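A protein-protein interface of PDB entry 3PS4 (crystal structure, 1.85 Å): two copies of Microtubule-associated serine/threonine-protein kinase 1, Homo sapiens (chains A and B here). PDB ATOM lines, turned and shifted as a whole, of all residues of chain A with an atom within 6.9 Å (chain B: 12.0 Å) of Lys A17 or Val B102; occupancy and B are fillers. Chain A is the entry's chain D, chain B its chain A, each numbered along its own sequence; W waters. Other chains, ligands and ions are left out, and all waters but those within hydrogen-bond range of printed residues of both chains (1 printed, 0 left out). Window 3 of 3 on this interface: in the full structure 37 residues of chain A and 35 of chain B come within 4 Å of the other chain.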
ATOM      1  N   GLN A  12       0.258  32.999  33.423  1.00  0.00           N
ATOM      2  CA  GLN A  12      -0.844  32.237  34.031  1.00  0.00           C
ATOM      3  C   GLN A  12      -1.699  31.615  32.951  1.00  0.00           C
ATOM      4  O   GLN A  12      -2.080  32.320  32.019  1.00  0.00           O
ATOM      5  CB  GLN A  12      -1.700  33.133  34.938  1.00  0.00           C
ATOM      6  CG  GLN A  12      -0.946  33.552  36.190  1.00  0.00           C
ATOM      7  CD  GLN A  12      -1.839  34.234  37.181  1.00  0.00           C
ATOM      8  OE1 GLN A  12      -1.840  35.462  37.300  1.00  0.00           O
ATOM      9  NE2 GLN A  12      -2.622  33.450  37.912  1.00  0.00           N
ATOM     10  N   ARG A  13      -2.003  30.308  33.061  1.00  0.00           N
ATOM     11  CA  ARG A  13      -2.815  29.591  32.062  1.00  0.00           C
ATOM     12  C   ARG A  13      -4.144  29.089  32.630  1.00  0.00           C
ATOM     13  O   ARG A  13      -4.213  28.734  33.806  1.00  0.00           O
ATOM     14  CB  ARG A  13      -2.036  28.422  31.452  1.00  0.00           C
ATOM     15  CG  ARG A  13      -1.567  27.341  32.417  1.00  0.00           C
ATOM     16  CD  ARG A  13      -0.831  26.250  31.659  1.00  0.00           C
ATOM     17  NE  ARG A  13      -0.140  25.304  32.543  1.00  0.00           N
ATOM     18  CZ  ARG A  13      -0.701  24.230  33.092  1.00  0.00           C
ATOM     19  NH1 ARG A  13      -1.983  23.970  32.896  1.00  0.00           N
ATOM     20  NH2 ARG A  13       0.012  23.423  33.866  1.00  0.00           N
ATOM     21  N   SER A  14      -5.197  29.058  31.786  1.00  0.00           N
ATOM     22  CA  SER A  14      -6.543  28.570  32.129  1.00  0.00           C
ATOM     23  C   SER A  14      -6.748  27.149  31.624  1.00  0.00           C
ATOM     24  O   SER A  14      -7.631  26.440  32.085  1.00  0.00           O
ATOM     25  CB  SER A  14      -7.621  29.475  31.536  1.00  0.00           C
ATOM     26  OG  SER A  14      -7.667  30.732  32.191  1.00  0.00           O
ATOM     27  N   GLY A  15      -5.967  26.779  30.628  1.00  0.00           N
ATOM     28  CA  GLY A  15      -6.012  25.459  30.021  1.00  0.00           C
ATOM     29  C   GLY A  15      -4.722  24.719  30.283  1.00  0.00           C
ATOM     30  O   GLY A  15      -3.991  25.044  31.225  1.00  0.00           O
ATOM     31  N   LYS A  16      -4.431  23.731  29.438  1.00  0.00           N
ATOM     32  CA  LYS A  16      -3.259  22.861  29.564  1.00  0.00           C
ATOM     33  C   LYS A  16      -1.941  23.542  29.233  1.00  0.00           C
ATOM     34  O   LYS A  16      -0.909  23.131  29.772  1.00  0.00           O
ATOM     35  CB  LYS A  16      -3.405  21.632  28.655  1.00  0.00           C
ATOM     36  CG  LYS A  16      -4.430  20.616  29.130  1.00  0.00           C
ATOM     37  CD  LYS A  16      -4.653  19.546  28.071  1.00  0.00           C
ATOM     38  N   LYS A  17      -1.940  24.539  28.325  1.00  0.00           N
ATOM     39  CA  LYS A  17      -0.680  25.120  27.881  1.00  0.00           C
ATOM     40  C   LYS A  17      -0.578  26.642  27.988  1.00  0.00           C
ATOM     41  O   LYS A  17      -1.566  27.370  27.969  1.00  0.00           O
ATOM     42  CB  LYS A  17      -0.400  24.691  26.425  1.00  0.00           C
ATOM     43  CG  LYS A  17       0.012  23.220  26.329  1.00  0.00           C
ATOM     44  CD  LYS A  17       0.236  22.746  24.917  1.00  0.00           C
ATOM     45  CE  LYS A  17       0.310  21.238  24.830  1.00  0.00           C
ATOM     46  NZ  LYS A  17       1.479  20.659  25.557  1.00  0.00           N
ATOM     47  N   TYR A  18       0.664  27.100  28.098  1.00  0.00           N
ATOM     48  CA  TYR A  18       1.031  28.508  28.190  1.00  0.00           C
ATOM     49  C   TYR A  18       0.999  29.214  26.836  1.00  0.00           C
ATOM     50  O   TYR A  18       0.978  30.442  26.801  1.00  0.00           O
ATOM     51  CB  TYR A  18       2.418  28.638  28.827  1.00  0.00           C
ATOM     52  CG  TYR A  18       2.348  28.391  30.316  1.00  0.00           C
ATOM     53  CD1 TYR A  18       1.674  29.270  31.157  1.00  0.00           C
ATOM     54  CD2 TYR A  18       2.911  27.252  30.881  1.00  0.00           C
ATOM     55  CE1 TYR A  18       1.573  29.034  32.526  1.00  0.00           C
ATOM     56  CE2 TYR A  18       2.807  26.997  32.251  1.00  0.00           C
ATOM     57  CZ  TYR A  18       2.127  27.889  33.070  1.00  0.00           C
ATOM     58  OH  TYR A  18       2.038  27.675  34.424  1.00  0.00           O
ATOM     59  N   GLY A  19       0.962  28.459  25.743  1.00  0.00           N
ATOM     60  CA  GLY A  19       0.909  29.073  24.418  1.00  0.00           C
ATOM     61  C   GLY A  19       2.245  29.533  23.870  1.00  0.00           C
ATOM     62  O   GLY A  19       2.344  30.602  23.256  1.00  0.00           O
ATOM     63  N   PHE A  20       3.294  28.734  24.076  1.00  0.00           N
ATOM     64  CA  PHE A  20       4.591  29.021  23.448  1.00  0.00           C
ATOM     65  C   PHE A  20       5.277  27.709  23.109  1.00  0.00           C
ATOM     66  O   PHE A  20       4.962  26.670  23.698  1.00  0.00           O
ATOM     67  CB  PHE A  20       5.507  29.977  24.257  1.00  0.00           C
ATOM     68  CG  PHE A  20       6.104  29.457  25.539  1.00  0.00           C
ATOM     69  CD1 PHE A  20       7.401  28.961  25.567  1.00  0.00           C
ATOM     70  CD2 PHE A  20       5.400  29.538  26.732  1.00  0.00           C
ATOM     71  CE1 PHE A  20       7.958  28.497  26.759  1.00  0.00           C
ATOM     72  CE2 PHE A  20       5.959  29.086  27.926  1.00  0.00           C
ATOM     73  CZ  PHE A  20       7.231  28.554  27.930  1.00  0.00           C
ATOM     74  N   THR A  21       6.142  27.752  22.097  1.00  0.00           N
ATOM     75  CA  THR A  21       6.917  26.612  21.624  1.00  0.00           C
ATOM     76  C   THR A  21       8.358  26.801  22.035  1.00  0.00           C
ATOM     77  O   THR A  21       8.950  27.852  21.779  1.00  0.00           O
ATOM     78  CB  THR A  21       6.791  26.442  20.110  1.00  0.00           C
ATOM     79  OG1 THR A  21       5.407  26.315  19.794  1.00  0.00           O
ATOM     80  CG2 THR A  21       7.565  25.214  19.591  1.00  0.00           C
ATOM     81  N   LEU A  22       8.920  25.767  22.642  1.00  0.00           N
ATOM     82  CA  LEU A  22      10.277  25.763  23.126  1.00  0.00           C
ATOM     83  C   LEU A  22      11.101  24.882  22.250  1.00  0.00           C
ATOM     84  O   LEU A  22      10.717  23.749  21.980  1.00  0.00           O
ATOM     85  CB  LEU A  22      10.281  25.269  24.585  1.00  0.00           C
ATOM     86  CG  LEU A  22      11.491  25.597  25.441  1.00  0.00           C
ATOM     87  CD1 LEU A  22      11.708  27.111  25.608  1.00  0.00           C
ATOM     88  CD2 LEU A  22      11.345  24.968  26.779  1.00  0.00           C
ATOM     89  N   GLU A  45       2.065  31.855  20.704  1.00  0.00           N
ATOM     90  CA  GLU A  45       0.743  31.842  20.079  1.00  0.00           C
ATOM     91  C   GLU A  45       0.042  33.168  20.282  1.00  0.00           C
ATOM     92  O   GLU A  45      -0.064  33.648  21.410  1.00  0.00           O
ATOM     93  CB  GLU A  45      -0.130  30.673  20.566  1.00  0.00           C
ATOM     94  CG  GLU A  45       0.478  29.315  20.217  1.00  0.00           C
ATOM     95  CD  GLU A  45       0.038  28.550  18.974  1.00  0.00           C
ATOM     96  OE1 GLU A  45       0.697  27.530  18.664  1.00  0.00           O
ATOM     97  OE2 GLU A  45      -0.942  28.965  18.308  1.00  0.00           O
ATOM     98  N   GLY A  48      -2.490  34.101  23.190  1.00  0.00           N
ATOM     99  CA  GLY A  48      -2.281  33.168  24.286  1.00  0.00           C
ATOM    100  C   GLY A  48      -1.725  33.798  25.547  1.00  0.00           C
ATOM    101  O   GLY A  48      -1.275  34.956  25.523  1.00  0.00           O
ATOM    102  N   PRO A  49      -1.685  33.014  26.650  1.00  0.00           N
ATOM    103  CA  PRO A  49      -1.161  33.543  27.925  1.00  0.00           C
ATOM    104  C   PRO A  49       0.270  34.097  27.837  1.00  0.00           C
ATOM    105  O   PRO A  49       0.526  35.161  28.416  1.00  0.00           O
ATOM    106  CB  PRO A  49      -1.223  32.319  28.861  1.00  0.00           C
ATOM    107  CG  PRO A  49      -2.230  31.402  28.268  1.00  0.00           C
ATOM    108  CD  PRO A  49      -2.170  31.618  26.793  1.00  0.00           C
ATOM    109  N   ALA A  50       1.196  33.391  27.134  1.00  0.00           N
ATOM    110  CA  ALA A  50       2.609  33.818  27.024  1.00  0.00           C
ATOM    111  C   ALA A  50       2.731  35.141  26.287  1.00  0.00           C
ATOM    112  O   ALA A  50       3.484  36.021  26.728  1.00  0.00           O
ATOM    113  CB  ALA A  50       3.461  32.740  26.343  1.00  0.00           C
ATOM    114  N   ILE A  61      15.213  31.249  27.268  1.00  0.00           N
ATOM    115  CA  ILE A  61      14.809  31.078  28.666  1.00  0.00           C
ATOM    116  C   ILE A  61      16.042  30.625  29.443  1.00  0.00           C
ATOM    117  O   ILE A  61      16.623  29.589  29.122  1.00  0.00           O
ATOM    118  CB  ILE A  61      13.622  30.088  28.782  1.00  0.00           C
ATOM    119  CG1 ILE A  61      12.330  30.735  28.156  1.00  0.00           C
ATOM    120  CG2 ILE A  61      13.395  29.659  30.260  1.00  0.00           C
ATOM    121  CD1 ILE A  61      11.164  29.820  28.039  1.00  0.00           C
ATOM    122  N   HIS A  74      16.090  19.376  26.707  1.00  0.00           N
ATOM    123  CA  HIS A  74      14.749  19.832  26.358  1.00  0.00           C
ATOM    124  C   HIS A  74      13.624  19.158  27.218  1.00  0.00           C
ATOM    125  O   HIS A  74      12.872  19.914  27.835  1.00  0.00           O
ATOM    126  CB  HIS A  74      14.497  19.640  24.865  1.00  0.00           C
ATOM    127  CG  HIS A  74      13.127  20.040  24.446  1.00  0.00           C
ATOM    128  ND1 HIS A  74      12.778  21.375  24.295  1.00  0.00           N
ATOM    129  CD2 HIS A  74      12.051  19.272  24.181  1.00  0.00           C
ATOM    130  CE1 HIS A  74      11.518  21.373  23.915  1.00  0.00           C
ATOM    131  NE2 HIS A  74      11.043  20.129  23.819  1.00  0.00           N
ATOM    132  N   VAL A  77      13.450  20.607  30.824  1.00  0.00           N
ATOM    133  CA  VAL A  77      12.929  21.979  30.916  1.00  0.00           C
ATOM    134  C   VAL A  77      11.416  21.958  30.743  1.00  0.00           C
ATOM    135  O   VAL A  77      10.715  22.669  31.465  1.00  0.00           O
ATOM    136  CB  VAL A  77      13.584  22.956  29.934  1.00  0.00           C
ATOM    137  CG1 VAL A  77      12.957  24.357  30.044  1.00  0.00           C
ATOM    138  CG2 VAL A  77      15.081  23.026  30.174  1.00  0.00           C
ATOM    139  N   VAL A  78      10.911  21.132  29.812  1.00  0.00           N
ATOM    140  CA  VAL A  78       9.475  20.980  29.564  1.00  0.00           C
ATOM    141  C   VAL A  78       8.804  20.482  30.862  1.00  0.00           C
ATOM    142  O   VAL A  78       7.771  21.025  31.245  1.00  0.00           O
ATOM    143  CB  VAL A  78       9.197  20.066  28.345  1.00  0.00           C
ATOM    144  CG1 VAL A  78       7.712  19.726  28.225  1.00  0.00           C
ATOM    145  CG2 VAL A  78       9.679  20.726  27.058  1.00  0.00           C
ATOM    146  N   GLU A  79       9.440  19.514  31.559  1.00  0.00           N
ATOM    147  CA  GLU A  79       8.966  18.941  32.829  1.00  0.00           C
ATOM    148  C   GLU A  79       8.909  20.018  33.928  1.00  0.00           C
ATOM    149  O   GLU A  79       7.930  20.043  34.675  1.00  0.00           O
ATOM    150  CB  GLU A  79       9.856  17.757  33.257  1.00  0.00           C
ATOM    151  CG  GLU A  79       9.410  17.011  34.508  1.00  0.00           C
ATOM    152  CD  GLU A  79       8.001  16.454  34.508  1.00  0.00           C
ATOM    153  OE1 GLU A  79       7.644  15.730  33.551  1.00  0.00           O
ATOM    154  OE2 GLU A  79       7.263  16.717  35.485  1.00  0.00           O
ATOM    155  N   ILE A  81       8.415  23.261  33.515  1.00  0.00           N
ATOM    156  CA  ILE A  81       7.279  24.112  33.154  1.00  0.00           C
ATOM    157  C   ILE A  81       5.980  23.361  33.471  1.00  0.00           C
ATOM    158  O   ILE A  81       5.083  23.948  34.071  1.00  0.00           O
ATOM    159  CB  ILE A  81       7.365  24.583  31.675  1.00  0.00           C
ATOM    160  CG1 ILE A  81       8.593  25.488  31.480  1.00  0.00           C
ATOM    161  CG2 ILE A  81       6.092  25.333  31.250  1.00  0.00           C
ATOM    162  CD1 ILE A  81       9.069  25.654  30.017  1.00  0.00           C
ATOM    163  N   LEU A  82       5.903  22.070  33.093  1.00  0.00           N
ATOM    164  CA  LEU A  82       4.746  21.202  33.318  1.00  0.00           C
ATOM    165  C   LEU A  82       4.396  21.051  34.811  1.00  0.00           C
ATOM    166  O   LEU A  82       3.212  21.111  35.151  1.00  0.00           O
ATOM    167  CB  LEU A  82       5.002  19.816  32.714  1.00  0.00           C
ATOM    168  N   THR B  98      14.061  19.718  17.725  1.00  0.00           N
ATOM    169  CA  THR B  98      13.615  19.324  19.072  1.00  0.00           C
ATOM    170  C   THR B  98      12.787  20.474  19.643  1.00  0.00           C
ATOM    171  O   THR B  98      13.342  21.492  20.087  1.00  0.00           O
ATOM    172  CB  THR B  98      14.813  18.977  19.988  1.00  0.00           C
ATOM    173  OG1 THR B  98      15.626  17.979  19.384  1.00  0.00           O
ATOM    174  CG2 THR B  98      14.388  18.503  21.377  1.00  0.00           C
ATOM    175  N   GLN B  99      11.464  20.325  19.586  1.00  0.00           N
ATOM    176  CA  GLN B  99      10.577  21.351  20.101  1.00  0.00           C
ATOM    177  C   GLN B  99       9.341  20.745  20.745  1.00  0.00           C
ATOM    178  O   GLN B  99       8.945  19.627  20.433  1.00  0.00           O
ATOM    179  CB  GLN B  99      10.191  22.391  19.030  1.00  0.00           C
ATOM    180  CG  GLN B  99       9.551  21.879  17.736  1.00  0.00           C
ATOM    181  CD  GLN B  99       9.533  22.984  16.694  1.00  0.00           C
ATOM    182  OE1 GLN B  99       8.487  23.511  16.318  1.00  0.00           O
ATOM    183  NE2 GLN B  99      10.696  23.405  16.238  1.00  0.00           N
ATOM    184  N   SER B 100       8.753  21.489  21.659  1.00  0.00           N
ATOM    185  CA  SER B 100       7.538  21.095  22.351  1.00  0.00           C
ATOM    186  C   SER B 100       6.653  22.293  22.554  1.00  0.00           C
ATOM    187  O   SER B 100       7.150  23.385  22.824  1.00  0.00           O
ATOM    188  CB  SER B 100       7.856  20.456  23.701  1.00  0.00           C
ATOM    189  OG  SER B 100       8.586  19.252  23.542  1.00  0.00           O
ATOM    190  N   LEU B 101       5.339  22.071  22.434  1.00  0.00           N
ATOM    191  CA  LEU B 101       4.312  23.056  22.683  1.00  0.00           C
ATOM    192  C   LEU B 101       4.052  23.019  24.172  1.00  0.00           C
ATOM    193  O   LEU B 101       3.709  21.969  24.713  1.00  0.00           O
ATOM    194  CB  LEU B 101       3.054  22.747  21.852  1.00  0.00           C
ATOM    195  CG  LEU B 101       2.991  23.376  20.447  1.00  0.00           C
ATOM    196  CD1 LEU B 101       4.070  22.821  19.522  1.00  0.00           C
ATOM    197  CD2 LEU B 101       1.616  23.133  19.812  1.00  0.00           C
ATOM    198  N   VAL B 102       4.309  24.131  24.853  1.00  0.00           N
ATOM    199  CA  VAL B 102       4.161  24.194  26.313  1.00  0.00           C
ATOM    200  C   VAL B 102       3.128  25.271  26.712  1.00  0.00           C
ATOM    201  O   VAL B 102       2.655  25.222  27.869  1.00  0.00           O
ATOM    202  CB  VAL B 102       5.530  24.399  27.022  1.00  0.00           C
ATOM    203  CG1 VAL B 102       6.303  23.089  27.108  1.00  0.00           C
ATOM    204  CG2 VAL B 102       6.362  25.459  26.327  1.00  0.00           C
ATOM    205  OXT VAL B 102       2.714  26.080  25.841  1.00  0.00           O
HETATM  206  O   HOH W   1       1.670  25.860  23.406  1.00  0.00           O
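The backbone carbonyl oxygen (O) of Ser B100 is in hydrogen-bond range of the backbone NH (N) of Leu A22 (3.0 Å).
OG of Ser B100 lies within hydrogen-bond range of NE2 of His A74, at 2.6 Å.
NZ of Lys A17 lies within hydrogen-bond range of O of Leu B101, 2.7 Å away.
O of Val B102 is in hydrogen-bond range of N of Tyr A18, 2.7 Å away.
The chain-end carboxylate (OXT) of Val B102 lies within hydrogen-bond range of the backbone NH (N) of Gly A19, 3.0 Å away.
The backbone NH of Val B102 is in hydrogen-bond range of the backbone carbonyl oxygen of Phe A20 (2.9 Å).
N of Ala A50 sits at hydrogen-bond distance from O of Tyr A18 (3.0 Å).
The backbone NH (N) of Glu A45 is in hydrogen-bond range of the backbone carbonyl oxygen (O) of Gly A19 (2.9 Å).
Among the printed residues, merely in contact across the chains: Leu A22 with Gln B99 (3.0 Å), Lys A17 with Val B102 (3.3 Å), Thr A21 with Ser B100 (3.5 Å), His A74 with Gln B99 (3.6 Å), His A74 with Thr B98 (3.7 Å), Thr A21 with Leu B101 (3.8 Å), Phe A20 with Leu B101 (3.8 Å), Thr A21 with Gln B99 (3.8 Å), Val A78 with Val B102 (3.8 Å), Val A78 with Ser B100 (3.8 Å) and Leu A22 with Thr B98 (3.9 Å).
No residue of chain B comes within 4 Å of Lys A16.
Of chain B, only Leu B101 (2.7 Å) and Val B102 (3.3 Å) come within 4 Å of Lys A17.
Of chain B, only Val B102 (2.7 Å) comes within 4 Å of Tyr A18.
Of the printed residues of chain B, Gly A19 touches Val B102.
Of the printed residues of chain B, Phe A20 touches Leu B101 (3.8 Å) and Val B102 (2.9 Å).
Of chain B, only Gln B99, Ser B100 and Leu B101 come within 4 Å of Thr A21.
Leu A22 touches three residues of chain B.
Glu A45 touches none of the printed residues of chain B.
Of the printed residues of chain B, His A74 touches Thr B98, Gln B99 and Ser B100.
Of chain B, only Ser B100 (3.8 Å) and Val B102 (3.8 Å) come within 4 Å of Val A78.
No residue of chain B comes within 4 Å of Ile A81.
Leu A82 touches none of the printed residues of chain B.
Of the printed residues of chain A, Thr B98 touches Leu A22 (3.9 Å) and His A74 (3.7 Å).
Of the printed residues of chain A, Gln B99 touches Thr A21 (3.8 Å), Leu A22 (3.0 Å) and His A74 (3.6 Å).
Of the printed residues of chain A, Leu B101 touches Lys A17 (2.7 Å), Phe A20 (3.8 Å) and Thr A21 (3.8 Å).
Val B102 touches just these residues of chain A: Lys A17 (3.3 Å), Tyr A18 (2.7 Å), Gly A19 (3.0 Å), Phe A20 (2.9 Å) and Val A78 (3.8 Å).
Of the 22 printed residues of chain A, 8 touch a printed residue of chain B.
Hydrophobic or aromatic side chains of chain A within 4 Å of the printed part of chain B: Tyr A18, Phe A20, His A74 and Val A78.
Along chain A the printed residues that touch a printed residue of chain B span positions 17 to 78.
Hydrophobic or aromatic side chains of chain B within 4 Å of the printed part of chain A: Leu B101 and Val B102.
Among the printed residues, 17 pairs touch across the chains.
Among the printed residues, no Asp or Glu carboxylate lies within 4 Å of a Lys or Arg side-chain nitrogen of the other chain.
No position is printed for both chains.
Of the 17 pairs that touch across the chains among the printed residues, none has its exchanged pair printed and touching as well.
Water W1 bridges OXT of Val B102 and N of Phe A20.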
